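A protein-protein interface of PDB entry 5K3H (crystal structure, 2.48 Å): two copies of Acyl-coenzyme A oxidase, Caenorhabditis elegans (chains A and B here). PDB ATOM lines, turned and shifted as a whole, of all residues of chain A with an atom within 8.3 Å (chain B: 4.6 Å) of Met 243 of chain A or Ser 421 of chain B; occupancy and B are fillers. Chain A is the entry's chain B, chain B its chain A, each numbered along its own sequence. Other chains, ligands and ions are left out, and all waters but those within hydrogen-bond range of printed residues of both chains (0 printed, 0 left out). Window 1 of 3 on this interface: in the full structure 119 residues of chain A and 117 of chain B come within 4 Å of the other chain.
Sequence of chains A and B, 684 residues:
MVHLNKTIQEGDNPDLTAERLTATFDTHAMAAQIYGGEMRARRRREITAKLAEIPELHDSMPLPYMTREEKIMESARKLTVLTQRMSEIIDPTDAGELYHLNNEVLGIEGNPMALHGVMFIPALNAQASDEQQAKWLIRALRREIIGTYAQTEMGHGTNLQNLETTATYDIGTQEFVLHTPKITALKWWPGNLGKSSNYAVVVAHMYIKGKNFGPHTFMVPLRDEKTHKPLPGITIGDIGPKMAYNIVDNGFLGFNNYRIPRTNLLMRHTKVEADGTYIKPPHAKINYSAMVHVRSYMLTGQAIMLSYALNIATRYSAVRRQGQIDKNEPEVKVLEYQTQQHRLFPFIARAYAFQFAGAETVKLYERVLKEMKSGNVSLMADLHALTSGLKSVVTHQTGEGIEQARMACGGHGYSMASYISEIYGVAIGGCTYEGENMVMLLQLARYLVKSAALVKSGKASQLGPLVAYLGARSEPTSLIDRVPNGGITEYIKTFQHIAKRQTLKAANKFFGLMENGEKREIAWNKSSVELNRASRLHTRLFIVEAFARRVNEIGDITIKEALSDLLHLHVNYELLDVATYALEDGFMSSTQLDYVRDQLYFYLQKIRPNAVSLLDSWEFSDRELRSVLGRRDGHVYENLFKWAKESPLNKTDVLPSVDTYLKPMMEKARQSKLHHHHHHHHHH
Tyr 414 of chain A touches Gly 425 of chain B, and with the chains exchanged Gly 425 of chain A touches Tyr 414 of chain B. Of the 16 pairs that touch across the chains among the printed residues, 2 have their exchanged pair printed and touching as well.
N of Tyr 245 of chain A lies within hydrogen-bond range of OE2 of Glu 422 of chain A, at 3.1 Å. The side-chain sulfur (SD) of Met 416 of chain B sits at hydrogen-bond distance from the side-chain hydroxyl (OG) of Ser 421 of chain B (3.3 Å). The backbone NH (N) of Lys 242 of chain A sits at hydrogen-bond distance from the side-chain amide oxygen (OD1) of Asn 246 of chain A. The side-chain amino group (NZ) of Lys 242 of chain A is in hydrogen-bond range of the backbone carbonyl oxygen (O) of Tyr 245 of chain A (2.8 Å).
The side-chain hydroxyl (OH) of Tyr 424 of chain B sits at hydrogen-bond distance from the side-chain carboxylate (OE2) of Glu 403 of chain A, 2.9 Å away. N of Met 243 of chain A lies within hydrogen-bond range of O of Tyr 414 of chain B (3.2 Å). The backbone carbonyl oxygen of Lys 242 of chain A sits close to the side-chain sulfur of Met 416 of chain B (3.8 Å). N of Met 416 of chain B lies within hydrogen-bond range of O of Pro 241 of chain A, 3.2 Å away. OH of Tyr 414 of chain B sits at hydrogen-bond distance from O of Gly 425 of chain A (2.7 Å). The backbone carbonyl oxygen (O) of Gly 425 of chain B lies within hydrogen-bond range of the side-chain hydroxyl (OH) of Tyr 414 of chain A, 2.6 Å away.
Printed residues of chain A that touch a printed residue of chain B: Trp 189, Pro 241, Lys 242, Met 243, Ala 244, Tyr 245, Glu 403, Tyr 414, Gly 425, Val 426, Ile 428 and Gly 429. Among the printed residues, no Asp or Glu carboxylate lies within 4 Å of a Lys or Arg side-chain nitrogen of the other chain.
Of chain A, only Met 243 comes within 4 Å of Ser 421 of chain B. Of the printed residues of chain A, Tyr 424 of chain B touches Glu 403. Of the printed residues of chain B, Glu 403 of chain A touches Tyr 424. Tyr 424 of chain A touches none of the printed residues of chain B. Ile 423 of chain B touches none of the printed residues of chain A. The nearest printed residue of chain B that does not touch Met 243 of chain A is Tyr 424 of chain B (6.3 Å). The nearest printed residue of chain A that does not touch Tyr 414 of chain B is Ile 428 of chain A (4.3 Å).
Among the printed residues, merely in contact across the chains: Trp 189 of chain A with Tyr 414 of chain B (3.9 Å), Lys 242 of chain A with Tyr 414 of chain B (3.8 Å), Met 243 of chain A with Arg 406 of chain B (3.8 Å), Met 243 of chain A with Met 416 of chain B (3.99 Å), Met 243 of chain A with Ser 421 of chain B (3.4 Å), Ala 244 of chain A with Tyr 414 of chain B (3.6 Å), Tyr 245 of chain A with Tyr 414 of chain B (3.6 Å), Val 426 of chain A with Tyr 414 of chain B (3.97 Å), Ile 428 of chain A with Arg 406 of chain B (3.6 Å) and Gly 429 of chain A with Tyr 414 of chain B (3.6 Å).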
ATOM      1  N   GLU A 109     -21.534  29.508   9.063  1.00  0.00           N
ATOM      2  CA  GLU A 109     -21.898  28.143   8.698  1.00  0.00           C
ATOM      3  C   GLU A 109     -20.700  27.261   8.343  1.00  0.00           C
ATOM      4  O   GLU A 109     -20.903  26.062   8.100  1.00  0.00           O
ATOM      5  CB  GLU A 109     -22.902  28.151   7.547  1.00  0.00           C
ATOM      6  CG  GLU A 109     -24.170  28.963   7.859  1.00  0.00           C
ATOM      7  CD  GLU A 109     -25.310  28.759   6.861  1.00  0.00           C
ATOM      8  OE1 GLU A 109     -25.378  27.656   6.275  1.00  0.00           O
ATOM      9  OE2 GLU A 109     -26.135  29.685   6.668  1.00  0.00           O
ATOM     10  N   TRP A 189     -16.146  12.948  13.288  1.00  0.00           N
ATOM     11  CA  TRP A 189     -16.463  14.349  13.631  1.00  0.00           C
ATOM     12  C   TRP A 189     -15.388  15.417  13.369  1.00  0.00           C
ATOM     13  O   TRP A 189     -15.756  16.601  13.377  1.00  0.00           O
ATOM     14  CB  TRP A 189     -16.918  14.492  15.103  1.00  0.00           C
ATOM     15  CG  TRP A 189     -18.365  14.154  15.252  1.00  0.00           C
ATOM     16  CD1 TRP A 189     -18.896  13.034  15.822  1.00  0.00           C
ATOM     17  CD2 TRP A 189     -19.473  14.923  14.760  1.00  0.00           C
ATOM     18  NE1 TRP A 189     -20.262  13.066  15.725  1.00  0.00           N
ATOM     19  CE2 TRP A 189     -20.641  14.215  15.076  1.00  0.00           C
ATOM     20  CE3 TRP A 189     -19.583  16.151  14.088  1.00  0.00           C
ATOM     21  CZ2 TRP A 189     -21.903  14.677  14.734  1.00  0.00           C
ATOM     22  CZ3 TRP A 189     -20.843  16.620  13.758  1.00  0.00           C
ATOM     23  CH2 TRP A 189     -21.989  15.882  14.078  1.00  0.00           C
ATOM     24  N   GLY A 240     -21.986  13.166   6.669  1.00  0.00           N
ATOM     25  CA  GLY A 240     -23.376  13.436   6.354  1.00  0.00           C
ATOM     26  C   GLY A 240     -23.868  14.795   6.833  1.00  0.00           C
ATOM     27  O   GLY A 240     -23.188  15.487   7.595  1.00  0.00           O
ATOM     28  N   PRO A 241     -25.092  15.163   6.453  1.00  0.00           N
ATOM     29  CA  PRO A 241     -25.629  16.473   6.836  1.00  0.00           C
ATOM     30  C   PRO A 241     -25.894  16.581   8.335  1.00  0.00           C
ATOM     31  O   PRO A 241     -25.997  15.585   9.062  1.00  0.00           O
ATOM     32  CB  PRO A 241     -26.932  16.571   6.031  1.00  0.00           C
ATOM     33  CG  PRO A 241     -27.351  15.120   5.861  1.00  0.00           C
ATOM     34  CD  PRO A 241     -26.073  14.357   5.697  1.00  0.00           C
ATOM     35  N   LYS A 242     -25.917  17.834   8.808  1.00  0.00           N
ATOM     36  CA  LYS A 242     -26.023  18.160  10.228  1.00  0.00           C
ATOM     37  C   LYS A 242     -27.132  19.179  10.467  1.00  0.00           C
ATOM     38  O   LYS A 242     -27.782  19.675   9.529  1.00  0.00           O
ATOM     39  CB  LYS A 242     -24.689  18.668  10.786  1.00  0.00           C
ATOM     40  CG  LYS A 242     -23.557  17.673  10.644  1.00  0.00           C
ATOM     41  CD  LYS A 242     -22.250  18.322  10.858  1.00  0.00           C
ATOM     42  CE  LYS A 242     -22.021  19.284   9.730  1.00  0.00           C
ATOM     43  NZ  LYS A 242     -20.815  20.097   9.909  1.00  0.00           N
ATOM     44  N   MET A 243     -27.361  19.468  11.756  1.00  0.00           N
ATOM     45  CA  MET A 243     -28.406  20.415  12.123  1.00  0.00           C
ATOM     46  C   MET A 243     -28.010  21.846  11.775  1.00  0.00           C
ATOM     47  O   MET A 243     -28.870  22.679  11.491  1.00  0.00           O
ATOM     48  CB  MET A 243     -28.761  20.270  13.608  1.00  0.00           C
ATOM     49  CG  MET A 243     -27.956  21.108  14.572  1.00  0.00           C
ATOM     50  SD  MET A 243     -28.522  20.868  16.279  1.00  0.00           S
ATOM     51  CE  MET A 243     -29.595  22.282  16.554  1.00  0.00           C
ATOM     52  N   ALA A 244     -26.726  22.140  11.745  1.00  0.00           N
ATOM     53  CA  ALA A 244     -26.259  23.452  11.326  1.00  0.00           C
ATOM     54  C   ALA A 244     -24.791  23.296  10.957  1.00  0.00           C
ATOM     55  O   ALA A 244     -24.246  22.187  10.977  1.00  0.00           O
ATOM     56  CB  ALA A 244     -26.492  24.506  12.421  1.00  0.00           C
ATOM     57  N   TYR A 245     -24.150  24.409  10.608  1.00  0.00           N
ATOM     58  CA  TYR A 245     -22.702  24.403  10.393  1.00  0.00           C
ATOM     59  C   TYR A 245     -22.318  23.495   9.223  1.00  0.00           C
ATOM     60  O   TYR A 245     -21.330  22.768   9.283  1.00  0.00           O
ATOM     61  CB  TYR A 245     -21.987  23.960  11.673  1.00  0.00           C
ATOM     62  CG  TYR A 245     -20.570  24.437  11.777  1.00  0.00           C
ATOM     63  CD1 TYR A 245     -20.278  25.787  11.641  1.00  0.00           C
ATOM     64  CD2 TYR A 245     -19.534  23.558  12.064  1.00  0.00           C
ATOM     65  CE1 TYR A 245     -18.990  26.253  11.751  1.00  0.00           C
ATOM     66  CE2 TYR A 245     -18.220  24.019  12.190  1.00  0.00           C
ATOM     67  CZ  TYR A 245     -17.960  25.372  12.027  1.00  0.00           C
ATOM     68  OH  TYR A 245     -16.677  25.867  12.141  1.00  0.00           O
ATOM     69  N   ASN A 246     -23.118  23.515   8.161  1.00  0.00           N
ATOM     70  CA  ASN A 246     -23.052  22.467   7.152  1.00  0.00           C
ATOM     71  C   ASN A 246     -22.048  22.737   6.040  1.00  0.00           C
ATOM     72  O   ASN A 246     -21.867  21.871   5.176  1.00  0.00           O
ATOM     73  CB  ASN A 246     -24.436  22.233   6.567  1.00  0.00           C
ATOM     74  CG  ASN A 246     -25.262  21.317   7.442  1.00  0.00           C
ATOM     75  OD1 ASN A 246     -24.890  20.160   7.644  1.00  0.00           O
ATOM     76  ND2 ASN A 246     -26.376  21.825   7.982  1.00  0.00           N
ATOM     77  N   GLU A 403     -32.378  31.250  21.923  1.00  0.00           N
ATOM     78  CA  GLU A 403     -33.728  30.707  21.777  1.00  0.00           C
ATOM     79  C   GLU A 403     -34.789  31.696  22.254  1.00  0.00           C
ATOM     80  O   GLU A 403     -35.801  31.897  21.570  1.00  0.00           O
ATOM     81  CB  GLU A 403     -33.849  29.392  22.546  1.00  0.00           C
ATOM     82  CG  GLU A 403     -35.062  28.551  22.188  1.00  0.00           C
ATOM     83  CD  GLU A 403     -35.057  28.054  20.742  1.00  0.00           C
ATOM     84  OE1 GLU A 403     -33.960  27.725  20.217  1.00  0.00           O
ATOM     85  OE2 GLU A 403     -36.154  28.002  20.118  1.00  0.00           O
ATOM     86  N   TYR A 414     -39.456  32.194  12.795  1.00  0.00           N
ATOM     87  CA  TYR A 414     -39.327  30.831  12.300  1.00  0.00           C
ATOM     88  C   TYR A 414     -38.740  30.788  10.901  1.00  0.00           C
ATOM     89  O   TYR A 414     -38.265  29.740  10.461  1.00  0.00           O
ATOM     90  CB  TYR A 414     -40.703  30.175  12.292  1.00  0.00           C
ATOM     91  CG  TYR A 414     -40.703  28.676  12.287  1.00  0.00           C
ATOM     92  CD1 TYR A 414     -40.459  27.968  13.447  1.00  0.00           C
ATOM     93  CD2 TYR A 414     -40.981  27.957  11.129  1.00  0.00           C
ATOM     94  CE1 TYR A 414     -40.470  26.580  13.458  1.00  0.00           C
ATOM     95  CE2 TYR A 414     -40.998  26.556  11.132  1.00  0.00           C
ATOM     96  CZ  TYR A 414     -40.746  25.883  12.302  1.00  0.00           C
ATOM     97  OH  TYR A 414     -40.757  24.508  12.339  1.00  0.00           O
ATOM     98  N   MET A 416     -36.105  31.516   7.805  1.00  0.00           N
ATOM     99  CA  MET A 416     -34.669  31.747   7.701  1.00  0.00           C
ATOM    100  C   MET A 416     -34.347  33.207   7.432  1.00  0.00           C
ATOM    101  O   MET A 416     -33.165  33.572   7.399  1.00  0.00           O
ATOM    102  CB  MET A 416     -34.021  30.879   6.639  1.00  0.00           C
ATOM    103  CG  MET A 416     -34.045  29.392   6.936  1.00  0.00           C
ATOM    104  SD  MET A 416     -33.469  28.880   8.578  1.00  0.00           S
ATOM    105  CE  MET A 416     -31.876  29.707   8.657  1.00  0.00           C
ATOM    106  N   SER A 421     -32.248  30.704  13.865  1.00  0.00           N
ATOM    107  CA  SER A 421     -32.164  29.258  14.027  1.00  0.00           C
ATOM    108  C   SER A 421     -30.797  28.714  13.641  1.00  0.00           C
ATOM    109  O   SER A 421     -30.319  27.756  14.261  1.00  0.00           O
ATOM    110  CB  SER A 421     -33.259  28.577  13.207  1.00  0.00           C
ATOM    111  OG  SER A 421     -33.042  28.745  11.819  1.00  0.00           O
ATOM    112  N   GLU A 422     -30.150  29.299  12.629  1.00  0.00           N
ATOM    113  CA  GLU A 422     -28.792  28.903  12.264  1.00  0.00           C
ATOM    114  C   GLU A 422     -27.781  29.456  13.261  1.00  0.00           C
ATOM    115  O   GLU A 422     -26.815  28.770  13.618  1.00  0.00           O
ATOM    116  CB  GLU A 422     -28.476  29.382  10.841  1.00  0.00           C
ATOM    117  CG  GLU A 422     -27.160  28.855  10.236  1.00  0.00           C
ATOM    118  CD  GLU A 422     -27.164  27.365   9.927  1.00  0.00           C
ATOM    119  OE1 GLU A 422     -28.256  26.772   9.765  1.00  0.00           O
ATOM    120  OE2 GLU A 422     -26.063  26.779   9.878  1.00  0.00           O
ATOM    121  N   TYR A 424     -28.376  29.845  16.398  1.00  0.00           N
ATOM    122  CA  TYR A 424     -28.501  28.908  17.512  1.00  0.00           C
ATOM    123  C   TYR A 424     -27.732  27.622  17.239  1.00  0.00           C
ATOM    124  O   TYR A 424     -26.990  27.128  18.096  1.00  0.00           O
ATOM    125  CB  TYR A 424     -29.986  28.606  17.768  1.00  0.00           C
ATOM    126  CG  TYR A 424     -30.260  27.552  18.834  1.00  0.00           C
ATOM    127  CD1 TYR A 424     -30.159  27.854  20.196  1.00  0.00           C
ATOM    128  CD2 TYR A 424     -30.623  26.257  18.478  1.00  0.00           C
ATOM    129  CE1 TYR A 424     -30.407  26.894  21.165  1.00  0.00           C
ATOM    130  CE2 TYR A 424     -30.874  25.292  19.448  1.00  0.00           C
ATOM    131  CZ  TYR A 424     -30.758  25.615  20.793  1.00  0.00           C
ATOM    132  OH  TYR A 424     -31.006  24.658  21.767  1.00  0.00           O
ATOM    133  N   GLY A 425     -27.939  27.035  16.064  1.00  0.00           N
ATOM    134  CA  GLY A 425     -27.340  25.740  15.771  1.00  0.00           C
ATOM    135  C   GLY A 425     -25.820  25.749  15.740  1.00  0.00           C
ATOM    136  O   GLY A 425     -25.171  24.772  16.129  1.00  0.00           O
ATOM    137  N   VAL A 426     -25.229  26.821  15.232  1.00  0.00           N
ATOM    138  CA  VAL A 426     -23.778  26.895  15.245  1.00  0.00           C
ATOM    139  C   VAL A 426     -23.274  27.093  16.672  1.00  0.00           C
ATOM    140  O   VAL A 426     -22.365  26.388  17.119  1.00  0.00           O
ATOM    141  CB  VAL A 426     -23.297  28.012  14.310  1.00  0.00           C
ATOM    142  CG1 VAL A 426     -21.781  28.126  14.391  1.00  0.00           C
ATOM    143  CG2 VAL A 426     -23.775  27.731  12.900  1.00  0.00           C
ATOM    144  N   ALA A 427     -23.872  28.037  17.421  1.00  0.00           N
ATOM    145  CA  ALA A 427     -23.433  28.297  18.799  1.00  0.00           C
ATOM    146  C   ALA A 427     -23.515  27.051  19.675  1.00  0.00           C
ATOM    147  O   ALA A 427     -22.647  26.819  20.520  1.00  0.00           O
ATOM    148  CB  ALA A 427     -24.254  29.417  19.421  1.00  0.00           C
ATOM    149  N   ILE A 428     -24.571  26.255  19.522  1.00  0.00           N
ATOM    150  CA  ILE A 428     -24.738  25.100  20.396  1.00  0.00           C
ATOM    151  C   ILE A 428     -23.817  23.951  19.988  1.00  0.00           C
ATOM    152  O   ILE A 428     -23.522  23.075  20.804  1.00  0.00           O
ATOM    153  CB  ILE A 428     -26.225  24.706  20.405  1.00  0.00           C
ATOM    154  CG1 ILE A 428     -26.635  24.319  21.814  1.00  0.00           C
ATOM    155  CG2 ILE A 428     -26.548  23.623  19.359  1.00  0.00           C
ATOM    156  CD1 ILE A 428     -26.698  25.523  22.768  1.00  0.00           C
ATOM    157  N   GLY A 429     -23.302  23.946  18.769  1.00  0.00           N
ATOM    158  CA  GLY A 429     -22.439  22.857  18.333  1.00  0.00           C
ATOM    159  C   GLY A 429     -20.987  23.007  18.757  1.00  0.00           C
ATOM    160  O   GLY A 429     -20.656  23.797  19.652  1.00  0.00           O
ATOM    161  N   ARG B 406     -31.502  15.712  22.686  1.00  0.00           N
ATOM    162  CA  ARG B 406     -30.429  15.870  21.714  1.00  0.00           C
ATOM    163  C   ARG B 406     -29.067  15.904  22.406  1.00  0.00           C
ATOM    164  O   ARG B 406     -28.132  15.195  21.999  1.00  0.00           O
ATOM    165  CB  ARG B 406     -30.653  17.135  20.882  1.00  0.00           C
ATOM    166  CG  ARG B 406     -29.757  17.216  19.660  1.00  0.00           C
ATOM    167  CD  ARG B 406     -29.800  18.570  19.014  1.00  0.00           C
ATOM    168  NE  ARG B 406     -29.525  19.635  19.965  1.00  0.00           N
ATOM    169  CZ  ARG B 406     -28.305  19.987  20.349  1.00  0.00           C
ATOM    170  NH1 ARG B 406     -27.249  19.349  19.858  1.00  0.00           N
ATOM    171  NH2 ARG B 406     -28.135  20.974  21.222  1.00  0.00           N
ATOM    172  N   TYR B 414     -25.924  15.790  17.123  1.00  0.00           N
ATOM    173  CA  TYR B 414     -25.876  16.942  16.221  1.00  0.00           C
ATOM    174  C   TYR B 414     -26.049  16.555  14.758  1.00  0.00           C
ATOM    175  O   TYR B 414     -26.371  17.418  13.935  1.00  0.00           O
ATOM    176  CB  TYR B 414     -24.535  17.661  16.421  1.00  0.00           C
ATOM    177  CG  TYR B 414     -24.417  19.074  15.887  1.00  0.00           C
ATOM    178  CD1 TYR B 414     -25.028  20.137  16.540  1.00  0.00           C
ATOM    179  CD2 TYR B 414     -23.607  19.359  14.778  1.00  0.00           C
ATOM    180  CE1 TYR B 414     -24.889  21.428  16.075  1.00  0.00           C
ATOM    181  CE2 TYR B 414     -23.462  20.648  14.305  1.00  0.00           C
ATOM    182  CZ  TYR B 414     -24.104  21.685  14.961  1.00  0.00           C
ATOM    183  OH  TYR B 414     -23.982  22.994  14.531  1.00  0.00           O
ATOM    184  N   MET B 416     -27.886  14.796  11.492  1.00  0.00           N
ATOM    185  CA  MET B 416     -29.265  14.471  11.123  1.00  0.00           C
ATOM    186  C   MET B 416     -29.582  12.985  11.270  1.00  0.00           C
ATOM    187  O   MET B 416     -30.760  12.618  11.228  1.00  0.00           O
ATOM    188  CB  MET B 416     -29.549  14.926   9.686  1.00  0.00           C
ATOM    189  CG  MET B 416     -29.483  16.432   9.499  1.00  0.00           C
ATOM    190  SD  MET B 416     -30.557  17.343  10.647  1.00  0.00           S
ATOM    191  CE  MET B 416     -32.126  16.545  10.285  1.00  0.00           C
ATOM    192  N   TYR B 419     -31.953  12.817  14.009  1.00  0.00           N
ATOM    193  CA  TYR B 419     -33.222  13.385  13.565  1.00  0.00           C
ATOM    194  C   TYR B 419     -33.855  14.296  14.620  1.00  0.00           C
ATOM    195  O   TYR B 419     -34.941  14.836  14.380  1.00  0.00           O
ATOM    196  CB  TYR B 419     -34.210  12.309  13.080  1.00  0.00           C
ATOM    197  CG  TYR B 419     -35.237  12.832  12.083  1.00  0.00           C
ATOM    198  CD1 TYR B 419     -34.837  13.518  10.917  1.00  0.00           C
ATOM    199  CD2 TYR B 419     -36.600  12.632  12.291  1.00  0.00           C
ATOM    200  CE1 TYR B 419     -35.774  14.011  10.000  1.00  0.00           C
ATOM    201  CE2 TYR B 419     -37.552  13.111  11.376  1.00  0.00           C
ATOM    202  CZ  TYR B 419     -37.139  13.808  10.240  1.00  0.00           C
ATOM    203  OH  TYR B 419     -38.095  14.285   9.348  1.00  0.00           O
ATOM    204  N   ILE B 420     -33.208  14.503  15.774  1.00  0.00           N
ATOM    205  CA  ILE B 420     -33.845  15.245  16.866  1.00  0.00           C
ATOM    206  C   ILE B 420     -33.951  16.742  16.566  1.00  0.00           C
ATOM    207  O   ILE B 420     -34.922  17.402  16.977  1.00  0.00           O
ATOM    208  CB  ILE B 420     -33.121  14.963  18.189  1.00  0.00           C
ATOM    209  CG1 ILE B 420     -33.318  13.485  18.552  1.00  0.00           C
ATOM    210  CG2 ILE B 420     -33.657  15.877  19.274  1.00  0.00           C
ATOM    211  CD1 ILE B 420     -32.588  13.026  19.770  1.00  0.00           C
ATOM    212  N   SER B 421     -33.004  17.301  15.807  1.00  0.00           N
ATOM    213  CA  SER B 421     -33.101  18.719  15.496  1.00  0.00           C
ATOM    214  C   SER B 421     -34.363  19.006  14.696  1.00  0.00           C
ATOM    215  O   SER B 421     -35.034  20.017  14.926  1.00  0.00           O
ATOM    216  CB  SER B 421     -31.868  19.191  14.728  1.00  0.00           C
ATOM    217  OG  SER B 421     -31.825  18.699  13.399  1.00  0.00           O
ATOM    218  N   GLU B 422     -34.758  18.086  13.810  1.00  0.00           N
ATOM    219  CA  GLU B 422     -36.006  18.296  13.076  1.00  0.00           C
ATOM    220  C   GLU B 422     -37.218  18.087  13.978  1.00  0.00           C
ATOM    221  O   GLU B 422     -38.207  18.814  13.874  1.00  0.00           O
ATOM    222  CB  GLU B 422     -36.068  17.373  11.859  1.00  0.00           C
ATOM    223  CG  GLU B 422     -37.225  17.671  10.908  1.00  0.00           C
ATOM    224  CD  GLU B 422     -37.095  19.006  10.211  1.00  0.00           C
ATOM    225  OE1 GLU B 422     -35.975  19.562  10.131  1.00  0.00           O
ATOM    226  OE2 GLU B 422     -38.129  19.504   9.718  1.00  0.00           O
ATOM    227  N   ILE B 423     -37.167  17.106  14.876  1.00  0.00           N
ATOM    228  CA  ILE B 423     -38.264  16.956  15.830  1.00  0.00           C
ATOM    229  C   ILE B 423     -38.419  18.225  16.664  1.00  0.00           C
ATOM    230  O   ILE B 423     -39.542  18.654  16.967  1.00  0.00           O
ATOM    231  CB  ILE B 423     -38.044  15.708  16.706  1.00  0.00           C
ATOM    232  CG1 ILE B 423     -38.087  14.442  15.831  1.00  0.00           C
ATOM    233  CG2 ILE B 423     -39.071  15.661  17.849  1.00  0.00           C
ATOM    234  CD1 ILE B 423     -37.466  13.257  16.455  1.00  0.00           C
ATOM    235  N   TYR B 424     -37.291  18.829  17.069  1.00  0.00           N
ATOM    236  CA  TYR B 424     -37.330  20.060  17.852  1.00  0.00           C
ATOM    237  C   TYR B 424     -37.955  21.212  17.062  1.00  0.00           C
ATOM    238  O   TYR B 424     -38.909  21.849  17.522  1.00  0.00           O
ATOM    239  CB  TYR B 424     -35.911  20.426  18.318  1.00  0.00           C
ATOM    240  CG  TYR B 424     -35.895  21.708  19.099  1.00  0.00           C
ATOM    241  CD1 TYR B 424     -36.318  21.735  20.414  1.00  0.00           C
ATOM    242  CD2 TYR B 424     -35.533  22.920  18.495  1.00  0.00           C
ATOM    243  CE1 TYR B 424     -36.355  22.930  21.130  1.00  0.00           C
ATOM    244  CE2 TYR B 424     -35.552  24.119  19.208  1.00  0.00           C
ATOM    245  CZ  TYR B 424     -35.967  24.109  20.520  1.00  0.00           C
ATOM    246  OH  TYR B 424     -36.008  25.284  21.233  1.00  0.00           O
ATOM    247  N   GLY B 425     -37.436  21.479  15.854  1.00  0.00           N
ATOM    248  CA  GLY B 425     -37.896  22.622  15.083  1.00  0.00           C
ATOM    249  C   GLY B 425     -39.367  22.544  14.720  1.00  0.00           C
ATOM    250  O   GLY B 425     -40.057  23.572  14.639  1.00  0.00           O
